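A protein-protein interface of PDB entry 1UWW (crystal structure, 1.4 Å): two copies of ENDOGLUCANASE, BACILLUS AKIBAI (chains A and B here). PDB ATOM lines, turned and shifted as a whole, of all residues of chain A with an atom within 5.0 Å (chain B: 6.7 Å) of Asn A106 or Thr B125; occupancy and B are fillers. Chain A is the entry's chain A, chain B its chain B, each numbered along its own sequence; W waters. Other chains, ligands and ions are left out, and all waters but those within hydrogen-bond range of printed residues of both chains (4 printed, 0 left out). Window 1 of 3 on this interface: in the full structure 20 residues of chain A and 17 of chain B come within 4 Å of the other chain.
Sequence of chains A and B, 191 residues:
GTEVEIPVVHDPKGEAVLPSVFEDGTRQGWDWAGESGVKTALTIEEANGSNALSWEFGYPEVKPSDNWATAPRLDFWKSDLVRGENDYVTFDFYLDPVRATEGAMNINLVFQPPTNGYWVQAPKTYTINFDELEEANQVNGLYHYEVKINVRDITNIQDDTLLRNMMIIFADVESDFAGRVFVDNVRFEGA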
ATOM      1  N   ALA A 104       5.046  33.359 -32.312  1.00  0.00           N
ATOM      2  CA  ALA A 104       6.130  32.752 -33.060  1.00  0.00           C
ATOM      3  C   ALA A 104       5.816  31.294 -33.300  1.00  0.00           C
ATOM      4  O   ALA A 104       4.831  30.760 -32.772  1.00  0.00           O
ATOM      5  CB  ALA A 104       7.473  32.939 -32.311  1.00  0.00           C
ATOM      6  N   MET A 105       6.661  30.658 -34.096  1.00  0.00           N
ATOM      7  CA  MET A 105       6.576  29.235 -34.405  1.00  0.00           C
ATOM      8  C   MET A 105       7.983  28.658 -34.222  1.00  0.00           C
ATOM      9  O   MET A 105       8.923  29.231 -34.779  1.00  0.00           O
ATOM     10  CB  MET A 105       6.149  29.054 -35.850  1.00  0.00           C
ATOM     11  CG  MET A 105       6.087  27.607 -36.332  1.00  0.00           C
ATOM     12  SD  MET A 105       5.654  27.436 -38.225  1.00  0.00           S
ATOM     13  CE  MET A 105       4.064  27.594 -37.957  1.00  0.00           C
ATOM     14  N   ASN A 106       8.110  27.547 -33.494  1.00  0.00           N
ATOM     15  CA  ASN A 106       9.366  26.851 -33.257  1.00  0.00           C
ATOM     16  C   ASN A 106       9.394  25.592 -34.090  1.00  0.00           C
ATOM     17  O   ASN A 106       8.532  24.708 -33.903  1.00  0.00           O
ATOM     18  CB  ASN A 106       9.527  26.471 -31.782  1.00  0.00           C
ATOM     19  CG  ASN A 106       9.969  27.626 -30.891  1.00  0.00           C
ATOM     20  OD1 ASN A 106       9.890  27.519 -29.638  1.00  0.00           O
ATOM     21  ND2 ASN A 106      10.449  28.680 -31.481  1.00  0.00           N
ATOM     22  N   ILE A 107      10.395  25.470 -34.952  1.00  0.00           N
ATOM     23  CA  ILE A 107      10.584  24.290 -35.788  1.00  0.00           C
ATOM     24  C   ILE A 107      11.688  23.418 -35.176  1.00  0.00           C
ATOM     25  O   ILE A 107      12.816  23.902 -34.949  1.00  0.00           O
ATOM     26  CB  ILE A 107      10.942  24.703 -37.236  1.00  0.00           C
ATOM     27  CG1 ILE A 107       9.807  25.561 -37.807  1.00  0.00           C
ATOM     28  CG2 ILE A 107      11.180  23.470 -38.073  1.00  0.00           C
ATOM     29  CD1 ILE A 107      10.075  26.053 -39.189  1.00  0.00           C
ATOM     30  N   ASN A 108      11.378  22.154 -34.885  1.00  0.00           N
ATOM     31  CA  ASN A 108      12.338  21.199 -34.362  1.00  0.00           C
ATOM     32  C   ASN A 108      12.463  19.997 -35.250  1.00  0.00           C
ATOM     33  O   ASN A 108      11.573  19.642 -36.003  1.00  0.00           O
ATOM     34  CB  ASN A 108      11.933  20.754 -32.952  1.00  0.00           C
ATOM     35  CG  ASN A 108      12.198  21.830 -31.889  1.00  0.00           C
ATOM     36  OD1 ASN A 108      11.267  22.441 -31.409  1.00  0.00           O
ATOM     37  ND2 ASN A 108      13.492  22.120 -31.616  1.00  0.00           N
ATOM     38  N   THR A 125      16.664  24.956 -31.868  1.00  0.00           N
ATOM     39  CA  THR A 125      15.378  25.259 -32.464  1.00  0.00           C
ATOM     40  C   THR A 125      15.482  26.378 -33.507  1.00  0.00           C
ATOM     41  O   THR A 125      16.231  27.334 -33.278  1.00  0.00           O
ATOM     42  CB  THR A 125      14.508  25.691 -31.313  1.00  0.00           C
ATOM     43  OG1 THR A 125      14.455  24.617 -30.359  1.00  0.00           O
ATOM     44  CG2 THR A 125      13.073  25.950 -31.764  1.00  0.00           C
ATOM     45  N   TYR A 126      14.768  26.262 -34.630  1.00  0.00           N
ATOM     46  CA  TYR A 126      14.641  27.316 -35.633  1.00  0.00           C
ATOM     47  C   TYR A 126      13.327  28.045 -35.379  1.00  0.00           C
ATOM     48  O   TYR A 126      12.256  27.458 -35.470  1.00  0.00           O
ATOM     49  CB  TYR A 126      14.658  26.750 -37.070  1.00  0.00           C
ATOM     50  CG  TYR A 126      14.687  27.826 -38.125  1.00  0.00           C
ATOM     51  CD1 TYR A 126      13.522  28.458 -38.525  1.00  0.00           C
ATOM     52  CD2 TYR A 126      15.900  28.276 -38.651  1.00  0.00           C
ATOM     53  CE1 TYR A 126      13.533  29.466 -39.455  1.00  0.00           C
ATOM     54  CE2 TYR A 126      15.934  29.304 -39.587  1.00  0.00           C
ATOM     55  CZ  TYR A 126      14.719  29.892 -39.991  1.00  0.00           C
ATOM     56  OH  TYR A 126      14.677  30.916 -40.913  1.00  0.00           O
ATOM     57  N   THR A 127      13.382  29.333 -35.125  1.00  0.00           N
ATOM     58  CA  THR A 127      12.227  30.088 -34.675  1.00  0.00           C
ATOM     59  C   THR A 127      11.857  31.160 -35.704  1.00  0.00           C
ATOM     60  O   THR A 127      12.732  31.921 -36.167  1.00  0.00           O
ATOM     61  CB  THR A 127      12.523  30.703 -33.294  1.00  0.00           C
ATOM     62  OG1 THR A 127      12.779  29.664 -32.351  1.00  0.00           O
ATOM     63  CG2 THR A 127      11.326  31.508 -32.764  1.00  0.00           C
ATOM     64  N   ILE A 169       8.733  19.161 -36.514  1.00  0.00           N
ATOM     65  CA  ILE A 169       7.660  19.611 -35.635  1.00  0.00           C
ATOM     66  C   ILE A 169       7.542  21.101 -35.748  1.00  0.00           C
ATOM     67  O   ILE A 169       8.537  21.815 -35.612  1.00  0.00           O
ATOM     68  CB  ILE A 169       7.973  19.195 -34.186  1.00  0.00           C
ATOM     69  CG1 ILE A 169       8.084  17.668 -34.082  1.00  0.00           C
ATOM     70  CG2 ILE A 169       6.847  19.695 -33.261  1.00  0.00           C
ATOM     71  CD1 ILE A 169       8.621  17.149 -32.786  1.00  0.00           C
ATOM     72  N   PHE A 170       6.332  21.604 -35.981  1.00  0.00           N
ATOM     73  CA  PHE A 170       6.055  23.028 -36.191  1.00  0.00           C
ATOM     74  C   PHE A 170       5.221  23.519 -35.018  1.00  0.00           C
ATOM     75  O   PHE A 170       3.975  23.467 -35.059  1.00  0.00           O
ATOM     76  CB  PHE A 170       5.325  23.251 -37.509  1.00  0.00           C
ATOM     77  CG  PHE A 170       6.109  22.835 -38.718  1.00  0.00           C
ATOM     78  CD1 PHE A 170       6.099  21.532 -39.146  1.00  0.00           C
ATOM     79  CD2 PHE A 170       6.859  23.755 -39.442  1.00  0.00           C
ATOM     80  CE1 PHE A 170       6.776  21.130 -40.285  1.00  0.00           C
ATOM     81  CE2 PHE A 170       7.558  23.360 -40.578  1.00  0.00           C
ATOM     82  CZ  PHE A 170       7.514  22.051 -40.991  1.00  0.00           C
ATOM     83  N   ALA A 171       5.855  23.973 -33.952  1.00  0.00           N
ATOM     84  CA  ALA A 171       5.156  24.242 -32.687  1.00  0.00           C
ATOM     85  C   ALA A 171       4.770  25.705 -32.507  1.00  0.00           C
ATOM     86  O   ALA A 171       5.508  26.615 -32.842  1.00  0.00           O
ATOM     87  CB  ALA A 171       6.023  23.806 -31.533  1.00  0.00           C
ATOM     88  N   VAL A 173       4.123  29.105 -30.526  1.00  0.00           N
ATOM     89  CA  VAL A 173       4.622  29.893 -29.409  1.00  0.00           C
ATOM     90  C   VAL A 173       3.723  31.124 -29.273  1.00  0.00           C
ATOM     91  O   VAL A 173       4.031  32.204 -29.751  1.00  0.00           O
ATOM     92  CB  VAL A 173       6.078  30.362 -29.640  1.00  0.00           C
ATOM     93  CG1 VAL A 173       6.622  31.010 -28.382  1.00  0.00           C
ATOM     94  CG2 VAL A 173       6.986  29.206 -30.091  1.00  0.00           C
ATOM     95  N   MET B 105      14.551  35.005 -27.559  1.00  0.00           N
ATOM     96  CA  MET B 105      15.524  34.186 -26.866  1.00  0.00           C
ATOM     97  C   MET B 105      14.916  32.816 -26.587  1.00  0.00           C
ATOM     98  O   MET B 105      13.795  32.727 -26.101  1.00  0.00           O
ATOM     99  CB  MET B 105      15.887  34.831 -25.529  1.00  0.00           C
ATOM    100  CG  MET B 105      16.757  33.972 -24.590  1.00  0.00           C
ATOM    101  SD  MET B 105      17.073  34.790 -22.819  1.00  0.00           S
ATOM    102  CE  MET B 105      18.107  35.532 -23.515  1.00  0.00           C
ATOM    103  N   ASN B 106      15.668  31.774 -26.891  1.00  0.00           N
ATOM    104  CA  ASN B 106      15.237  30.394 -26.638  1.00  0.00           C
ATOM    105  C   ASN B 106      15.981  29.822 -25.462  1.00  0.00           C
ATOM    106  O   ASN B 106      17.208  29.889 -25.441  1.00  0.00           O
ATOM    107  CB  ASN B 106      15.491  29.520 -27.861  1.00  0.00           C
ATOM    108  CG  ASN B 106      14.439  29.720 -28.949  1.00  0.00           C
ATOM    109  OD1 ASN B 106      13.380  30.247 -28.687  1.00  0.00           O
ATOM    110  ND2 ASN B 106      14.764  29.344 -30.174  1.00  0.00           N
ATOM    111  N   ILE B 107      15.263  29.244 -24.520  1.00  0.00           N
ATOM    112  CA  ILE B 107      15.835  28.620 -23.324  1.00  0.00           C
ATOM    113  C   ILE B 107      15.637  27.091 -23.412  1.00  0.00           C
ATOM    114  O   ILE B 107      14.531  26.597 -23.609  1.00  0.00           O
ATOM    115  CB  ILE B 107      15.231  29.184 -22.032  1.00  0.00           C
ATOM    116  CG1 ILE B 107      15.317  30.717 -22.046  1.00  0.00           C
ATOM    117  CG2 ILE B 107      15.883  28.471 -20.816  1.00  0.00           C
ATOM    118  CD1 ILE B 107      14.762  31.377 -20.819  1.00  0.00           C
ATOM    119  N   ASN B 108      16.746  26.366 -23.290  1.00  0.00           N
ATOM    120  CA  ASN B 108      16.767  24.900 -23.391  1.00  0.00           C
ATOM    121  C   ASN B 108      17.454  24.303 -22.172  1.00  0.00           C
ATOM    122  O   ASN B 108      18.314  24.926 -21.549  1.00  0.00           O
ATOM    123  CB  ASN B 108      17.425  24.444 -24.697  1.00  0.00           C
ATOM    124  CG  ASN B 108      16.566  24.754 -25.920  1.00  0.00           C
ATOM    125  OD1 ASN B 108      16.811  25.760 -26.600  1.00  0.00           O
ATOM    126  ND2 ASN B 108      15.514  23.968 -26.141  1.00  0.00           N
ATOM    127  N   GLN B 121      18.205  16.058 -23.881  1.00  0.00           N
ATOM    128  CA  GLN B 121      17.626  17.395 -23.885  1.00  0.00           C
ATOM    129  C   GLN B 121      16.141  17.334 -23.653  1.00  0.00           C
ATOM    130  O   GLN B 121      15.441  16.493 -24.223  1.00  0.00           O
ATOM    131  CB  GLN B 121      17.915  18.049 -25.228  1.00  0.00           C
ATOM    132  CG  GLN B 121      17.677  19.565 -25.276  1.00  0.00           C
ATOM    133  CD  GLN B 121      18.252  20.216 -26.544  1.00  0.00           C
ATOM    134  OE1 GLN B 121      17.778  21.277 -26.987  1.00  0.00           O
ATOM    135  NE2 GLN B 121      19.273  19.598 -27.107  1.00  0.00           N
ATOM    136  N   ALA B 122      15.625  18.229 -22.829  1.00  0.00           N
ATOM    137  CA  ALA B 122      14.185  18.390 -22.735  1.00  0.00           C
ATOM    138  C   ALA B 122      13.696  18.762 -24.133  1.00  0.00           C
ATOM    139  O   ALA B 122      14.250  19.658 -24.772  1.00  0.00           O
ATOM    140  CB  ALA B 122      13.810  19.438 -21.741  1.00  0.00           C
ATOM    141  N   PRO B 123      12.690  18.072 -24.653  1.00  0.00           N
ATOM    142  CA  PRO B 123      12.308  18.266 -26.058  1.00  0.00           C
ATOM    143  C   PRO B 123      11.786  19.654 -26.406  1.00  0.00           C
ATOM    144  O   PRO B 123      12.068  20.128 -27.511  1.00  0.00           O
ATOM    145  CB  PRO B 123      11.224  17.204 -26.271  1.00  0.00           C
ATOM    146  CG  PRO B 123      10.723  16.865 -24.931  1.00  0.00           C
ATOM    147  CD  PRO B 123      11.924  16.972 -24.024  1.00  0.00           C
ATOM    148  N   LYS B 124      11.069  20.304 -25.508  1.00  0.00           N
ATOM    149  CA  LYS B 124      10.442  21.575 -25.819  1.00  0.00           C
ATOM    150  C   LYS B 124      11.271  22.780 -25.340  1.00  0.00           C
ATOM    151  O   LYS B 124      11.952  22.751 -24.316  1.00  0.00           O
ATOM    152  CB  LYS B 124       9.023  21.583 -25.289  1.00  0.00           C
ATOM    153  CG  LYS B 124       8.199  20.518 -25.950  1.00  0.00           C
ATOM    154  CD  LYS B 124       6.831  20.408 -25.338  1.00  0.00           C
ATOM    155  CE  LYS B 124       6.277  19.011 -25.435  1.00  0.00           C
ATOM    156  NZ  LYS B 124       5.577  18.692 -24.167  1.00  0.00           N
ATOM    157  N   THR B 125      11.276  23.806 -26.174  1.00  0.00           N
ATOM    158  CA  THR B 125      11.998  25.052 -25.953  1.00  0.00           C
ATOM    159  C   THR B 125      11.093  26.047 -25.293  1.00  0.00           C
ATOM    160  O   THR B 125       9.909  26.128 -25.655  1.00  0.00           O
ATOM    161  CB  THR B 125      12.389  25.580 -27.337  1.00  0.00           C
ATOM    162  OG1 THR B 125      13.248  24.623 -27.937  1.00  0.00           O
ATOM    163  CG2 THR B 125      13.182  26.895 -27.291  1.00  0.00           C
ATOM    164  N   TYR B 126      11.603  26.803 -24.337  1.00  0.00           N
ATOM    165  CA  TYR B 126      10.874  27.924 -23.761  1.00  0.00           C
ATOM    166  C   TYR B 126      11.336  29.209 -24.470  1.00  0.00           C
ATOM    167  O   TYR B 126      12.510  29.533 -24.434  1.00  0.00           O
ATOM    168  CB  TYR B 126      11.110  27.996 -22.238  1.00  0.00           C
ATOM    169  CG  TYR B 126      10.256  29.055 -21.600  1.00  0.00           C
ATOM    170  CD1 TYR B 126      10.652  30.377 -21.592  1.00  0.00           C
ATOM    171  CD2 TYR B 126       9.047  28.731 -21.002  1.00  0.00           C
ATOM    172  CE1 TYR B 126       9.880  31.346 -21.043  1.00  0.00           C
ATOM    173  CE2 TYR B 126       8.239  29.725 -20.441  1.00  0.00           C
ATOM    174  CZ  TYR B 126       8.673  31.033 -20.468  1.00  0.00           C
ATOM    175  OH  TYR B 126       7.892  32.036 -19.925  1.00  0.00           O
ATOM    176  N   THR B 127      10.424  29.934 -25.095  1.00  0.00           N
ATOM    177  CA  THR B 127      10.772  31.087 -25.920  1.00  0.00           C
ATOM    178  C   THR B 127      10.255  32.387 -25.320  1.00  0.00           C
ATOM    179  O   THR B 127       9.100  32.476 -24.904  1.00  0.00           O
ATOM    180  CB  THR B 127      10.185  30.881 -27.334  1.00  0.00           C
ATOM    181  OG1 THR B 127      10.799  29.741 -27.938  1.00  0.00           O
ATOM    182  CG2 THR B 127      10.490  32.070 -28.238  1.00  0.00           C
ATOM    183  N   LYS B 148       9.301  27.183 -17.319  1.00  0.00           N
ATOM    184  CA  LYS B 148       8.847  25.860 -16.942  1.00  0.00           C
ATOM    185  C   LYS B 148       9.127  24.946 -18.122  1.00  0.00           C
ATOM    186  O   LYS B 148       8.615  25.170 -19.221  1.00  0.00           O
ATOM    187  CB  LYS B 148       7.373  25.880 -16.568  1.00  0.00           C
ATOM    188  CG  LYS B 148       6.884  24.584 -15.981  1.00  0.00           C
ATOM    189  CD  LYS B 148       5.648  24.820 -15.125  1.00  0.00           C
ATOM    190  CE  LYS B 148       5.050  23.527 -14.605  1.00  0.00           C
ATOM    191  NZ  LYS B 148       3.692  23.777 -13.999  1.00  0.00           N
ATOM    192  N   ILE B 149       9.955  23.933 -17.895  1.00  0.00           N
ATOM    193  CA  ILE B 149      10.406  23.034 -18.953  1.00  0.00           C
ATOM    194  C   ILE B 149      10.096  21.593 -18.541  1.00  0.00           C
ATOM    195  O   ILE B 149      10.520  21.133 -17.482  1.00  0.00           O
ATOM    196  CB  ILE B 149      11.895  23.205 -19.256  1.00  0.00           C
ATOM    197  CG1 ILE B 149      12.146  24.638 -19.778  1.00  0.00           C
ATOM    198  CG2 ILE B 149      12.359  22.134 -20.256  1.00  0.00           C
ATOM    199  CD1 ILE B 149      13.587  25.080 -19.770  1.00  0.00           C
ATOM    200  N   VAL B 173      17.751  34.467 -30.799  1.00  0.00           N
ATOM    201  CA  VAL B 173      16.977  34.339 -32.045  1.00  0.00           C
ATOM    202  C   VAL B 173      16.841  35.717 -32.711  1.00  0.00           C
ATOM    203  O   VAL B 173      15.839  36.405 -32.549  1.00  0.00           O
ATOM    204  CB  VAL B 173      15.567  33.758 -31.774  1.00  0.00           C
ATOM    205  CG1 VAL B 173      14.845  33.478 -33.078  1.00  0.00           C
ATOM    206  CG2 VAL B 173      15.621  32.507 -30.913  1.00  0.00           C
HETATM  207  O   HOH W   1      11.644  22.626 -28.750  1.00  0.00           O
HETATM  208  O   HOH W   2      17.367  28.355 -30.908  1.00  0.00           O
HETATM  209  O   HOH W   3      15.837  21.655 -29.759  1.00  0.00           O
HETATM  210  O   HOH W   4       8.531  25.342 -28.366  1.00  0.00           O
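OD1 of Asn B106 is in hydrogen-bond range of OG1 of Thr B127 (2.7 Å).
OG1 of Thr A125 lies within hydrogen-bond range of ND2 of Asn A108 (3.0 Å).
N of Val A173 sits at hydrogen-bond distance from O of Ala A104 (2.9 Å).
The backbone NH (N) of Ala A171 sits at hydrogen-bond distance from the backbone carbonyl oxygen (O) of Asn A106, at 2.8 Å.
The side-chain amide nitrogen (ND2) of Asn A106 is in hydrogen-bond range of the side-chain hydroxyl (OG1) of Thr A127 (2.7 Å).
The side-chain amide nitrogen (ND2) of Asn B108 lies within hydrogen-bond range of the side-chain hydroxyl (OG1) of Thr B125 (3.0 Å).
Printed residues of chain A that touch a printed residue of chain B: Asn A106, Thr A125, Thr A127 and Val A173.
Hydrophobic or aromatic side chains of chain A that line the printed part of chain B: Val A173.
Of the 14 printed residues of chain B, 4 touch a printed residue of chain A.
Hydrophobic or aromatic side chains of chain B within 4 Å of the printed part of chain A: Val B173.
Among the printed residues, 7 pairs touch across the chains.
Among the printed residues, no Asp or Glu carboxylate lies within 4 Å of a Lys or Arg side-chain nitrogen of the other chain.
Water W1 lies within hydrogen-bond range of OG1 of Thr B125, OD1 of Asn A108 and O of Pro B123.
Water W2 lies within hydrogen-bond range of O of Thr A125 and ND2 of Asn B106.
Water W4 lies within hydrogen-bond range of the side-chain amide oxygen (OD1) of Asn A106 (2.9 Å) and the backbone carbonyl oxygen (O) of Thr B125 (3.1 Å).
Water W3 lies within hydrogen-bond range of the side-chain amide nitrogen (ND2) of Asn A108, the side-chain hydroxyl (OG1) of Thr A125 and the side-chain amide oxygen (OE1) of Gln B121.
Asn A106 touches Thr B125, and with the chains exchanged Thr A125 touches Asn B106.
Asn A106 touches Thr B127, and with the chains exchanged Thr A127 touches Asn B106.
Thr B125 touches its own counterpart, Thr A125.
Thr A127 touches Val B173, and with the chains exchanged Val A173 touches Thr B127.
Of the 7 pairs that touch across the chains among the printed residues, 7 have their exchanged pair printed and touching as well.
OD1 of Asn A106 lies within hydrogen-bond range of OG1 of Thr B127 (2.9 Å).
OG1 of Thr A127 sits at hydrogen-bond distance from ND2 of Asn B106.
The side-chain hydroxyl (OG1) of Thr A125 is in hydrogen-bond range of the side-chain hydroxyl (OG1) of Thr B125, at 2.7 Å.
OD1 of Asn A106 touches CB of Thr B125, at 3.9 Å.
Thr A125 touches Asn B106 (CB to ND2, 3.8 Å).
Val B173 touches Thr A127.
Thr B127 touches Val A173 (CB to CG1, 3.7 Å).
Of the printed residues of chain B, Asn A106 touches Thr B125 and Thr B127.
Thr B125 touches just these residues of chain A: Asn A106 (3.9 Å) and Thr A125 (2.7 Å).
Printed residues of chain A within 4 Å of Asn B106: Thr A125 and Thr A127.
Printed residues of chain A within 4 Å of Val B173: Thr A127.
Of the printed residues of chain B, Thr A125 touches Asn B106 and Thr B125.
Printed residues of chain B within 4 Å of Thr A127: Asn B106 and Val B173.
Of the printed residues of chain B, Val A173 touches Thr B127 (3.7 Å).
Pro B123 touches none of the printed residues of chain A.
Met B105 touches none of the printed residues of chain A.
The nearest residue of chain A that does not touch Thr B125 is Asn A108 (4.5 Å).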
